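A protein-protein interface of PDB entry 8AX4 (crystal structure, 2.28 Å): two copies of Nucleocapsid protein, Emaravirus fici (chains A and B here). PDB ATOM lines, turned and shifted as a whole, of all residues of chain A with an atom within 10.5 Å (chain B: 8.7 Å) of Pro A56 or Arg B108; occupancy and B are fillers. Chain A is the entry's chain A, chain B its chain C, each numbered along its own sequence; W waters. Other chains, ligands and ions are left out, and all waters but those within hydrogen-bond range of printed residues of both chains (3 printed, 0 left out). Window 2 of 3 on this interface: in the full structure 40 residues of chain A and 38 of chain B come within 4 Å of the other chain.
The backbone carbonyl oxygen of Ile B110 sits at hydrogen-bond distance from a ring nitrogen (NE2) of His B91, at 2.9 Å.
The backbone NH of Val B119 lies within hydrogen-bond range of the backbone carbonyl oxygen of Leu B107 (2.8 Å).
O of Leu B109 is in hydrogen-bond range of N of Leu B117 (2.8 Å).
The backbone carbonyl oxygen of His B91 lies within hydrogen-bond range of the side-chain amide nitrogen of Asn B98, 2.9 Å away.
No position is printed for both chains.
Of the 15 pairs that touch across the chains among the printed residues, none has its exchanged pair printed and touching as well.
Hydrophobic or aromatic side chains of chain B that line the printed part of chain A: His B91, Leu B107 and Leu B109.
Along chain B the printed residues that touch a printed residue of chain A span positions 91 to 109.
Of the 11 printed residues of chain A, 7 touch a printed residue of chain B.
Printed residues of chain A that touch a printed residue of chain B: Leu A54, Lys A55, Pro A56, Ile A57, Asp A58, Val A59 and Val A61.
Hydrophobic or aromatic side chains of chain A that line the printed part of chain B: Leu A54, Pro A56, Ile A57, Val A59 and Val A61.
Along chain A the printed residues that touch a printed residue of chain B span positions 54 to 61.
Among the printed residues, 15 pairs touch across the chains.
Among the printed residues, Asp or Glu carboxylates within 4 Å of a Lys or Arg side-chain nitrogen of the other chain: Asp A58 with Arg B108.
Printed residues of chain B within 4 Å of Pro A56: Asn B106, Leu B107 and Arg B108.
Arg B108 touches just these residues of chain A: Pro A56 (3.7 Å), Ile A57 (2.9 Å), Asp A58 (2.5 Å) and Val A59 (3.2 Å).
Leu B107 touches just these residues of chain A: Pro A56 and Ile A57.
Of chain A, only Val A59 (3.6 Å) comes within 4 Å of Leu B109.
Of the printed residues of chain B, Leu A54 touches Asn B106.
Printed residues of chain A within 4 Å of Asn B98: Val A59.
Val B118 touches none of the printed residues of chain A.
Ala A104 touches none of the printed residues of chain B.
The nearest printed residue of chain B that does not touch Ile A57 is Leu B109 (5.5 Å).
Among the printed residues, pairs that only touch across the chains: Pro A56 with Asn B106 (3.3 Å), Pro A56 with Leu B107 (3.7 Å), Pro A56 with Arg B108 (3.7 Å), Ile A57 with Arg B105 (3.5 Å), Ile A57 with Leu B107 (3.7 Å), Val A59 with His B91 (3.9 Å), Val A59 with Asn B98 (3.8 Å), Val A59 with Leu B109 (3.6 Å) and Val A61 with His B91 (3.6 Å).
Water W1 lies within hydrogen-bond range of NE of Arg B105, O of Lys A55 and N of Asn B106.
Water W2 lies within hydrogen-bond range of the backbone NH (N) of Ile B110 (2.7 Å) and the backbone carbonyl oxygen (O) of Val A59 (2.7 Å).
Water W3 lies within hydrogen-bond range of the side-chain carboxylate of Asp A58 and the backbone carbonyl oxygen of Arg B108.
O of Lys A55 lies within hydrogen-bond range of NH2 of Arg B105, 2.8 Å away.
The backbone carbonyl oxygen (O) of Ile A57 lies within hydrogen-bond range of the backbone NH (N) of Arg B108, 2.9 Å away.
The backbone carbonyl oxygen (O) of Asn B106 is in hydrogen-bond range of the backbone NH (N) of Ile A57 (2.9 Å).
The backbone carbonyl oxygen (O) of Leu A54 is in hydrogen-bond range of the side-chain amide nitrogen (ND2) of Asn B106, 3.0 Å away.
The side-chain carboxylate of Asp A58 is in salt-bridge range of the guanidinium group of Arg B108 (2.5 Å).
The backbone NH of Val A59 sits at hydrogen-bond distance from the backbone carbonyl oxygen of Arg B108 (3.2 Å).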
ATOM      1  N   LEU A  54     -37.480  35.880 -17.651  1.00  0.00           N
ATOM      2  CA  LEU A  54     -36.273  35.524 -16.916  1.00  0.00           C
ATOM      3  C   LEU A  54     -35.031  35.971 -17.677  1.00  0.00           C
ATOM      4  O   LEU A  54     -33.925  35.953 -17.132  1.00  0.00           O
ATOM      5  CB  LEU A  54     -36.226  34.017 -16.659  1.00  0.00           C
ATOM      6  CG  LEU A  54     -37.147  33.478 -15.563  1.00  0.00           C
ATOM      7  CD1 LEU A  54     -37.210  31.958 -15.613  1.00  0.00           C
ATOM      8  CD2 LEU A  54     -36.689  33.950 -14.192  1.00  0.00           C
ATOM      9  N   LYS A  55     -35.238  36.375 -18.938  1.00  0.00           N
ATOM     10  CA  LYS A  55     -34.229  36.841 -19.888  1.00  0.00           C
ATOM     11  C   LYS A  55     -32.880  36.165 -19.678  1.00  0.00           C
ATOM     12  O   LYS A  55     -31.895  36.836 -19.340  1.00  0.00           O
ATOM     13  CB  LYS A  55     -34.064  38.360 -19.795  1.00  0.00           C
ATOM     14  CG  LYS A  55     -35.369  39.133 -19.819  1.00  0.00           C
ATOM     15  CD  LYS A  55     -35.164  40.561 -19.344  1.00  0.00           C
ATOM     16  CE  LYS A  55     -34.566  40.594 -17.946  1.00  0.00           C
ATOM     17  NZ  LYS A  55     -34.416  41.985 -17.438  1.00  0.00           N
ATOM     18  N   PRO A  56     -32.787  34.854 -19.871  1.00  0.00           N
ATOM     19  CA  PRO A  56     -31.510  34.174 -19.660  1.00  0.00           C
ATOM     20  C   PRO A  56     -30.559  34.426 -20.815  1.00  0.00           C
ATOM     21  O   PRO A  56     -30.969  34.611 -21.962  1.00  0.00           O
ATOM     22  CB  PRO A  56     -31.901  32.691 -19.583  1.00  0.00           C
ATOM     23  CG  PRO A  56     -33.360  32.611 -20.008  1.00  0.00           C
ATOM     24  CD  PRO A  56     -33.782  33.965 -20.488  1.00  0.00           C
ATOM     25  N   ILE A  57     -29.276  34.449 -20.495  1.00  0.00           N
ATOM     26  CA  ILE A  57     -28.247  34.493 -21.525  1.00  0.00           C
ATOM     27  C   ILE A  57     -27.926  33.067 -21.939  1.00  0.00           C
ATOM     28  O   ILE A  57     -27.913  32.148 -21.110  1.00  0.00           O
ATOM     29  CB  ILE A  57     -26.986  35.236 -21.039  1.00  0.00           C
ATOM     30  CG1 ILE A  57     -26.413  34.591 -19.774  1.00  0.00           C
ATOM     31  CG2 ILE A  57     -27.283  36.712 -20.815  1.00  0.00           C
ATOM     32  CD1 ILE A  57     -24.991  35.023 -19.468  1.00  0.00           C
ATOM     33  N   ASP A  58     -27.696  32.874 -23.233  1.00  0.00           N
ATOM     34  CA  ASP A  58     -27.272  31.577 -23.735  1.00  0.00           C
ATOM     35  C   ASP A  58     -25.800  31.373 -23.411  1.00  0.00           C
ATOM     36  O   ASP A  58     -24.978  32.270 -23.626  1.00  0.00           O
ATOM     37  CB  ASP A  58     -27.504  31.485 -25.242  1.00  0.00           C
ATOM     38  CG  ASP A  58     -28.966  31.635 -25.617  1.00  0.00           C
ATOM     39  OD1 ASP A  58     -29.781  30.791 -25.190  1.00  0.00           O
ATOM     40  OD2 ASP A  58     -29.301  32.599 -26.338  1.00  0.00           O
ATOM     41  N   VAL A  59     -25.467  30.203 -22.878  1.00  0.00           N
ATOM     42  CA  VAL A  59     -24.096  29.870 -22.516  1.00  0.00           C
ATOM     43  C   VAL A  59     -23.601  28.819 -23.498  1.00  0.00           C
ATOM     44  O   VAL A  59     -24.062  27.670 -23.482  1.00  0.00           O
ATOM     45  CB  VAL A  59     -23.986  29.379 -21.068  1.00  0.00           C
ATOM     46  CG1 VAL A  59     -22.542  29.037 -20.737  1.00  0.00           C
ATOM     47  CG2 VAL A  59     -24.517  30.435 -20.111  1.00  0.00           C
ATOM     48  N   GLU A  60     -22.669  29.217 -24.359  1.00  0.00           N
ATOM     49  CA  GLU A  60     -22.088  28.297 -25.325  1.00  0.00           C
ATOM     50  C   GLU A  60     -21.338  27.183 -24.608  1.00  0.00           C
ATOM     51  O   GLU A  60     -20.515  27.439 -23.725  1.00  0.00           O
ATOM     52  CB  GLU A  60     -21.144  29.057 -26.257  1.00  0.00           C
ATOM     53  CG  GLU A  60     -20.911  28.404 -27.607  1.00  0.00           C
ATOM     54  CD  GLU A  60     -19.763  29.042 -28.364  1.00  0.00           C
ATOM     55  OE1 GLU A  60     -18.767  29.429 -27.716  1.00  0.00           O
ATOM     56  OE2 GLU A  60     -19.856  29.161 -29.604  1.00  0.00           O
ATOM     57  N   VAL A  61     -21.640  25.936 -24.982  1.00  0.00           N
ATOM     58  CA  VAL A  61     -20.888  24.806 -24.449  1.00  0.00           C
ATOM     59  C   VAL A  61     -19.444  24.903 -24.919  1.00  0.00           C
ATOM     60  O   VAL A  61     -19.174  25.060 -26.115  1.00  0.00           O
ATOM     61  CB  VAL A  61     -21.534  23.478 -24.878  1.00  0.00           C
ATOM     62  CG1 VAL A  61     -21.109  22.359 -23.950  1.00  0.00           C
ATOM     63  CG2 VAL A  61     -23.048  23.600 -24.903  1.00  0.00           C
ATOM     64  N   GLN A  62     -18.506  24.826 -23.969  1.00  0.00           N
ATOM     65  CA  GLN A  62     -17.083  24.848 -24.307  1.00  0.00           C
ATOM     66  C   GLN A  62     -16.326  24.196 -23.149  1.00  0.00           C
ATOM     67  O   GLN A  62     -16.093  24.841 -22.123  1.00  0.00           O
ATOM     68  CB  GLN A  62     -16.606  26.266 -24.566  1.00  0.00           C
ATOM     69  CG  GLN A  62     -15.107  26.386 -24.803  1.00  0.00           C
ATOM     70  CD  GLN A  62     -14.755  26.465 -26.277  1.00  0.00           C
ATOM     71  OE1 GLN A  62     -15.598  26.784 -27.119  1.00  0.00           O
ATOM     72  NE2 GLN A  62     -13.505  26.163 -26.596  1.00  0.00           N
ATOM     73  N   GLN A 103     -19.852  39.391 -17.728  1.00  0.00           N
ATOM     74  CA  GLN A 103     -20.478  38.077 -17.650  1.00  0.00           C
ATOM     75  C   GLN A 103     -21.308  37.775 -18.889  1.00  0.00           C
ATOM     76  O   GLN A 103     -21.425  36.611 -19.291  1.00  0.00           O
ATOM     77  CB  GLN A 103     -21.343  37.980 -16.393  1.00  0.00           C
ATOM     78  CG  GLN A 103     -20.588  38.256 -15.105  1.00  0.00           C
ATOM     79  CD  GLN A 103     -19.247  37.547 -15.053  1.00  0.00           C
ATOM     80  OE1 GLN A 103     -19.166  36.333 -15.243  1.00  0.00           O
ATOM     81  NE2 GLN A 103     -18.187  38.304 -14.798  1.00  0.00           N
ATOM     82  N   ALA A 104     -21.879  38.803 -19.516  1.00  0.00           N
ATOM     83  CA  ALA A 104     -22.741  38.630 -20.679  1.00  0.00           C
ATOM     84  C   ALA A 104     -22.015  38.833 -22.002  1.00  0.00           C
ATOM     85  O   ALA A 104     -22.245  38.074 -22.948  1.00  0.00           O
ATOM     86  CB  ALA A 104     -23.930  39.592 -20.601  1.00  0.00           C
ATOM     87  N   HIS B  91     -20.529  21.448 -19.503  1.00  0.00           N
ATOM     88  CA  HIS B  91     -21.131  22.429 -18.604  1.00  0.00           C
ATOM     89  C   HIS B  91     -20.612  22.258 -17.183  1.00  0.00           C
ATOM     90  O   HIS B  91     -20.324  23.244 -16.494  1.00  0.00           O
ATOM     91  CB  HIS B  91     -22.653  22.305 -18.627  1.00  0.00           C
ATOM     92  CG  HIS B  91     -23.295  22.892 -19.845  1.00  0.00           C
ATOM     93  ND1 HIS B  91     -22.994  24.153 -20.311  1.00  0.00           N
ATOM     94  CD2 HIS B  91     -24.231  22.393 -20.686  1.00  0.00           C
ATOM     95  CE1 HIS B  91     -23.713  24.404 -21.391  1.00  0.00           C
ATOM     96  NE2 HIS B  91     -24.473  23.353 -21.639  1.00  0.00           N
ATOM     97  N   ASN B  98     -19.812  29.210 -14.839  1.00  0.00           N
ATOM     98  CA  ASN B  98     -21.269  29.292 -14.845  1.00  0.00           C
ATOM     99  C   ASN B  98     -21.776  29.981 -13.586  1.00  0.00           C
ATOM    100  O   ASN B  98     -22.742  30.751 -13.634  1.00  0.00           O
ATOM    101  CB  ASN B  98     -21.881  27.896 -14.970  1.00  0.00           C
ATOM    102  CG  ASN B  98     -21.553  27.226 -16.290  1.00  0.00           C
ATOM    103  OD1 ASN B  98     -21.347  27.891 -17.305  1.00  0.00           O
ATOM    104  ND2 ASN B  98     -21.509  25.898 -16.283  1.00  0.00           N
ATOM    105  N   LEU B 102     -23.869  33.516 -13.352  1.00  0.00           N
ATOM    106  CA  LEU B 102     -25.211  33.524 -12.774  1.00  0.00           C
ATOM    107  C   LEU B 102     -25.384  34.672 -11.786  1.00  0.00           C
ATOM    108  O   LEU B 102     -26.512  35.079 -11.490  1.00  0.00           O
ATOM    109  CB  LEU B 102     -25.514  32.181 -12.107  1.00  0.00           C
ATOM    110  CG  LEU B 102     -26.913  31.977 -11.516  1.00  0.00           C
ATOM    111  CD1 LEU B 102     -27.945  31.830 -12.618  1.00  0.00           C
ATOM    112  CD2 LEU B 102     -26.929  30.754 -10.622  1.00  0.00           C
ATOM    113  N   ARG B 105     -26.626  37.334 -14.464  1.00  0.00           N
ATOM    114  CA  ARG B 105     -27.785  37.003 -15.281  1.00  0.00           C
ATOM    115  C   ARG B 105     -28.202  35.558 -15.051  1.00  0.00           C
ATOM    116  O   ARG B 105     -27.425  34.732 -14.568  1.00  0.00           O
ATOM    117  CB  ARG B 105     -27.500  37.211 -16.775  1.00  0.00           C
ATOM    118  CG  ARG B 105     -26.930  38.572 -17.124  1.00  0.00           C
ATOM    119  CD  ARG B 105     -28.035  39.602 -17.220  1.00  0.00           C
ATOM    120  NE  ARG B 105     -29.117  39.143 -18.083  1.00  0.00           N
ATOM    121  CZ  ARG B 105     -29.165  39.360 -19.393  1.00  0.00           C
ATOM    122  NH1 ARG B 105     -28.190  40.033 -19.990  1.00  0.00           N
ATOM    123  NH2 ARG B 105     -30.186  38.906 -20.106  1.00  0.00           N
ATOM    124  N   ASN B 106     -29.449  35.263 -15.410  1.00  0.00           N
ATOM    125  CA  ASN B 106     -29.898  33.883 -15.481  1.00  0.00           C
ATOM    126  C   ASN B 106     -29.280  33.201 -16.699  1.00  0.00           C
ATOM    127  O   ASN B 106     -28.891  33.849 -17.675  1.00  0.00           O
ATOM    128  CB  ASN B 106     -31.423  33.816 -15.547  1.00  0.00           C
ATOM    129  CG  ASN B 106     -32.083  34.311 -14.275  1.00  0.00           C
ATOM    130  OD1 ASN B 106     -31.519  34.203 -13.186  1.00  0.00           O
ATOM    131  ND2 ASN B 106     -33.285  34.860 -14.407  1.00  0.00           N
ATOM    132  N   LEU B 107     -29.192  31.876 -16.637  1.00  0.00           N
ATOM    133  CA  LEU B 107     -28.486  31.100 -17.646  1.00  0.00           C
ATOM    134  C   LEU B 107     -29.441  30.165 -18.373  1.00  0.00           C
ATOM    135  O   LEU B 107     -30.357  29.601 -17.767  1.00  0.00           O
ATOM    136  CB  LEU B 107     -27.355  30.282 -17.014  1.00  0.00           C
ATOM    137  CG  LEU B 107     -26.401  31.037 -16.089  1.00  0.00           C
ATOM    138  CD1 LEU B 107     -25.269  30.129 -15.639  1.00  0.00           C
ATOM    139  CD2 LEU B 107     -25.855  32.275 -16.780  1.00  0.00           C
ATOM    140  N   ARG B 108     -29.224  30.011 -19.677  1.00  0.00           N
ATOM    141  CA  ARG B 108     -29.833  28.943 -20.459  1.00  0.00           C
ATOM    142  C   ARG B 108     -28.731  27.979 -20.875  1.00  0.00           C
ATOM    143  O   ARG B 108     -27.807  28.365 -21.599  1.00  0.00           O
ATOM    144  CB  ARG B 108     -30.569  29.480 -21.688  1.00  0.00           C
ATOM    145  CG  ARG B 108     -31.278  28.382 -22.476  1.00  0.00           C
ATOM    146  CD  ARG B 108     -31.891  28.874 -23.781  1.00  0.00           C
ATOM    147  NE  ARG B 108     -33.014  29.785 -23.577  1.00  0.00           N
ATOM    148  CZ  ARG B 108     -32.960  31.099 -23.771  1.00  0.00           C
ATOM    149  NH1 ARG B 108     -31.835  31.668 -24.182  1.00  0.00           N
ATOM    150  NH2 ARG B 108     -34.036  31.845 -23.559  1.00  0.00           N
ATOM    151  N   LEU B 109     -28.825  26.736 -20.410  1.00  0.00           N
ATOM    152  CA  LEU B 109     -27.848  25.699 -20.716  1.00  0.00           C
ATOM    153  C   LEU B 109     -28.507  24.637 -21.587  1.00  0.00           C
ATOM    154  O   LEU B 109     -29.429  23.949 -21.139  1.00  0.00           O
ATOM    155  CB  LEU B 109     -27.295  25.064 -19.441  1.00  0.00           C
ATOM    156  CG  LEU B 109     -26.568  25.953 -18.433  1.00  0.00           C
ATOM    157  CD1 LEU B 109     -25.953  25.102 -17.336  1.00  0.00           C
ATOM    158  CD2 LEU B 109     -25.505  26.787 -19.119  1.00  0.00           C
ATOM    159  N   ILE B 110     -28.034  24.509 -22.822  1.00  0.00           N
ATOM    160  CA  ILE B 110     -28.472  23.425 -23.692  1.00  0.00           C
ATOM    161  C   ILE B 110     -27.784  22.144 -23.243  1.00  0.00           C
ATOM    162  O   ILE B 110     -26.552  22.087 -23.156  1.00  0.00           O
ATOM    163  CB  ILE B 110     -28.155  23.741 -25.162  1.00  0.00           C
ATOM    164  CG1 ILE B 110     -28.797  25.071 -25.566  1.00  0.00           C
ATOM    165  CG2 ILE B 110     -28.603  22.599 -26.066  1.00  0.00           C
ATOM    166  CD1 ILE B 110     -30.246  24.965 -25.972  1.00  0.00           C
ATOM    167  N   VAL B 111     -28.576  21.117 -22.944  1.00  0.00           N
ATOM    168  CA  VAL B 111     -28.040  19.854 -22.455  1.00  0.00           C
ATOM    169  C   VAL B 111     -28.130  18.737 -23.489  1.00  0.00           C
ATOM    170  O   VAL B 111     -27.358  17.770 -23.397  1.00  0.00           O
ATOM    171  CB  VAL B 111     -28.727  19.428 -21.142  1.00  0.00           C
ATOM    172  CG1 VAL B 111     -28.402  20.420 -20.035  1.00  0.00           C
ATOM    173  CG2 VAL B 111     -30.228  19.323 -21.336  1.00  0.00           C
ATOM    174  N   GLU B 115     -33.318  19.291 -25.226  1.00  0.00           N
ATOM    175  CA  GLU B 115     -33.573  19.816 -23.893  1.00  0.00           C
ATOM    176  C   GLU B 115     -32.601  20.934 -23.554  1.00  0.00           C
ATOM    177  O   GLU B 115     -31.458  20.956 -24.018  1.00  0.00           O
ATOM    178  CB  GLU B 115     -33.476  18.716 -22.829  1.00  0.00           C
ATOM    179  CG  GLU B 115     -34.593  17.682 -22.875  1.00  0.00           C
ATOM    180  CD  GLU B 115     -35.956  18.256 -22.530  1.00  0.00           C
ATOM    181  OE1 GLU B 115     -36.035  19.429 -22.101  1.00  0.00           O
ATOM    182  OE2 GLU B 115     -36.957  17.528 -22.691  1.00  0.00           O
ATOM    183  N   PHE B 116     -33.078  21.860 -22.723  1.00  0.00           N
ATOM    184  CA  PHE B 116     -32.247  22.887 -22.115  1.00  0.00           C
ATOM    185  C   PHE B 116     -32.753  23.140 -20.702  1.00  0.00           C
ATOM    186  O   PHE B 116     -33.901  22.838 -20.368  1.00  0.00           O
ATOM    187  CB  PHE B 116     -32.252  24.193 -22.923  1.00  0.00           C
ATOM    188  CG  PHE B 116     -33.602  24.851 -23.010  1.00  0.00           C
ATOM    189  CD1 PHE B 116     -34.515  24.462 -23.977  1.00  0.00           C
ATOM    190  CD2 PHE B 116     -33.956  25.863 -22.132  1.00  0.00           C
ATOM    191  CE1 PHE B 116     -35.756  25.064 -24.062  1.00  0.00           C
ATOM    192  CE2 PHE B 116     -35.196  26.468 -22.212  1.00  0.00           C
ATOM    193  CZ  PHE B 116     -36.096  26.068 -23.179  1.00  0.00           C
ATOM    194  N   LEU B 117     -31.875  23.691 -19.870  1.00  0.00           N
ATOM    195  CA  LEU B 117     -32.227  24.098 -18.520  1.00  0.00           C
ATOM    196  C   LEU B 117     -32.057  25.605 -18.387  1.00  0.00           C
ATOM    197  O   LEU B 117     -31.161  26.199 -18.994  1.00  0.00           O
ATOM    198  CB  LEU B 117     -31.359  23.393 -17.469  1.00  0.00           C
ATOM    199  CG  LEU B 117     -31.406  21.867 -17.381  1.00  0.00           C
ATOM    200  CD1 LEU B 117     -30.283  21.359 -16.490  1.00  0.00           C
ATOM    201  CD2 LEU B 117     -32.755  21.390 -16.864  1.00  0.00           C
ATOM    202  N   VAL B 118     -32.931  26.219 -17.596  1.00  0.00           N
ATOM    203  CA  VAL B 118     -32.803  27.622 -17.224  1.00  0.00           C
ATOM    204  C   VAL B 118     -32.385  27.669 -15.763  1.00  0.00           C
ATOM    205  O   VAL B 118     -33.115  27.195 -14.884  1.00  0.00           O
ATOM    206  CB  VAL B 118     -34.105  28.401 -17.462  1.00  0.00           C
ATOM    207  CG1 VAL B 118     -33.932  29.856 -17.053  1.00  0.00           C
ATOM    208  CG2 VAL B 118     -34.525  28.298 -18.920  1.00  0.00           C
ATOM    209  N   VAL B 119     -31.146  28.105 -15.559  1.00  0.00           N
ATOM    210  CA  VAL B 119     -30.545  28.151 -14.202  1.00  0.00           C
ATOM    211  C   VAL B 119     -30.780  29.544 -13.636  1.00  0.00           C
ATOM    212  O   VAL B 119     -30.568  30.516 -14.357  1.00  0.00           O
ATOM    213  CB  VAL B 119     -29.054  27.792 -14.275  1.00  0.00           C
ATOM    214  CG1 VAL B 119     -28.434  27.627 -12.901  1.00  0.00           C
ATOM    215  CG2 VAL B 119     -28.816  26.565 -15.134  1.00  0.00           C
ATOM    216  N   VAL B 120     -31.252  29.611 -12.400  1.00  0.00           N
ATOM    217  CA  VAL B 120     -31.628  30.922 -11.812  1.00  0.00           C
ATOM    218  C   VAL B 120     -31.309  30.946 -10.320  1.00  0.00           C
ATOM    219  O   VAL B 120     -31.196  29.863  -9.744  1.00  0.00           O
ATOM    220  CB  VAL B 120     -33.128  31.204 -12.070  1.00  0.00           C
ATOM    221  CG1 VAL B 120     -33.859  30.068 -12.766  1.00  0.00           C
ATOM    222  CG2 VAL B 120     -33.912  31.628 -10.840  1.00  0.00           C
ATOM    223  N   ASN B 130     -37.913  22.712 -16.198  1.00  0.00           N
ATOM    224  CA  ASN B 130     -36.615  23.123 -16.798  1.00  0.00           C
ATOM    225  C   ASN B 130     -36.013  24.337 -16.084  1.00  0.00           C
ATOM    226  O   ASN B 130     -34.855  24.640 -16.345  1.00  0.00           O
ATOM    227  CB  ASN B 130     -36.740  23.314 -18.309  1.00  0.00           C
ATOM    228  CG  ASN B 130     -37.421  24.603 -18.700  1.00  0.00           C
ATOM    229  OD1 ASN B 130     -38.524  24.894 -18.249  1.00  0.00           O
ATOM    230  ND2 ASN B 130     -36.769  25.380 -19.543  1.00  0.00           N
ATOM    231  N   VAL B 131     -36.780  24.993 -15.218  1.00  0.00           N
ATOM    232  CA  VAL B 131     -36.261  26.156 -14.446  1.00  0.00           C
ATOM    233  C   VAL B 131     -35.729  25.636 -13.109  1.00  0.00           C
ATOM    234  O   VAL B 131     -36.536  25.218 -12.286  1.00  0.00           O
ATOM    235  CB  VAL B 131     -37.309  27.277 -14.337  1.00  0.00           C
ATOM    236  CG1 VAL B 131     -36.799  28.473 -13.561  1.00  0.00           C
ATOM    237  CG2 VAL B 131     -37.812  27.707 -15.703  1.00  0.00           C
ATOM    238  N   MET B 141     -27.149  17.395 -14.463  1.00  0.00           N
ATOM    239  CA  MET B 141     -26.148  17.099 -15.482  1.00  0.00           C
ATOM    240  C   MET B 141     -25.144  16.060 -14.999  1.00  0.00           C
ATOM    241  O   MET B 141     -24.657  15.255 -15.800  1.00  0.00           O
ATOM    242  CB  MET B 141     -25.438  18.385 -15.903  1.00  0.00           C
ATOM    243  CG  MET B 141     -26.358  19.371 -16.605  1.00  0.00           C
ATOM    244  SD  MET B 141     -25.522  20.855 -17.188  1.00  0.00           S
ATOM    245  CE  MET B 141     -24.987  21.577 -15.639  1.00  0.00           C
HETATM  246  O   HOH W   1     -30.781  37.535 -16.862  1.00  0.00           O
HETATM  247  O   HOH W   2     -26.064  25.911 -23.908  1.00  0.00           O
HETATM  248  O   HOH W   3     -28.593  28.186 -24.501  1.00  0.00           O
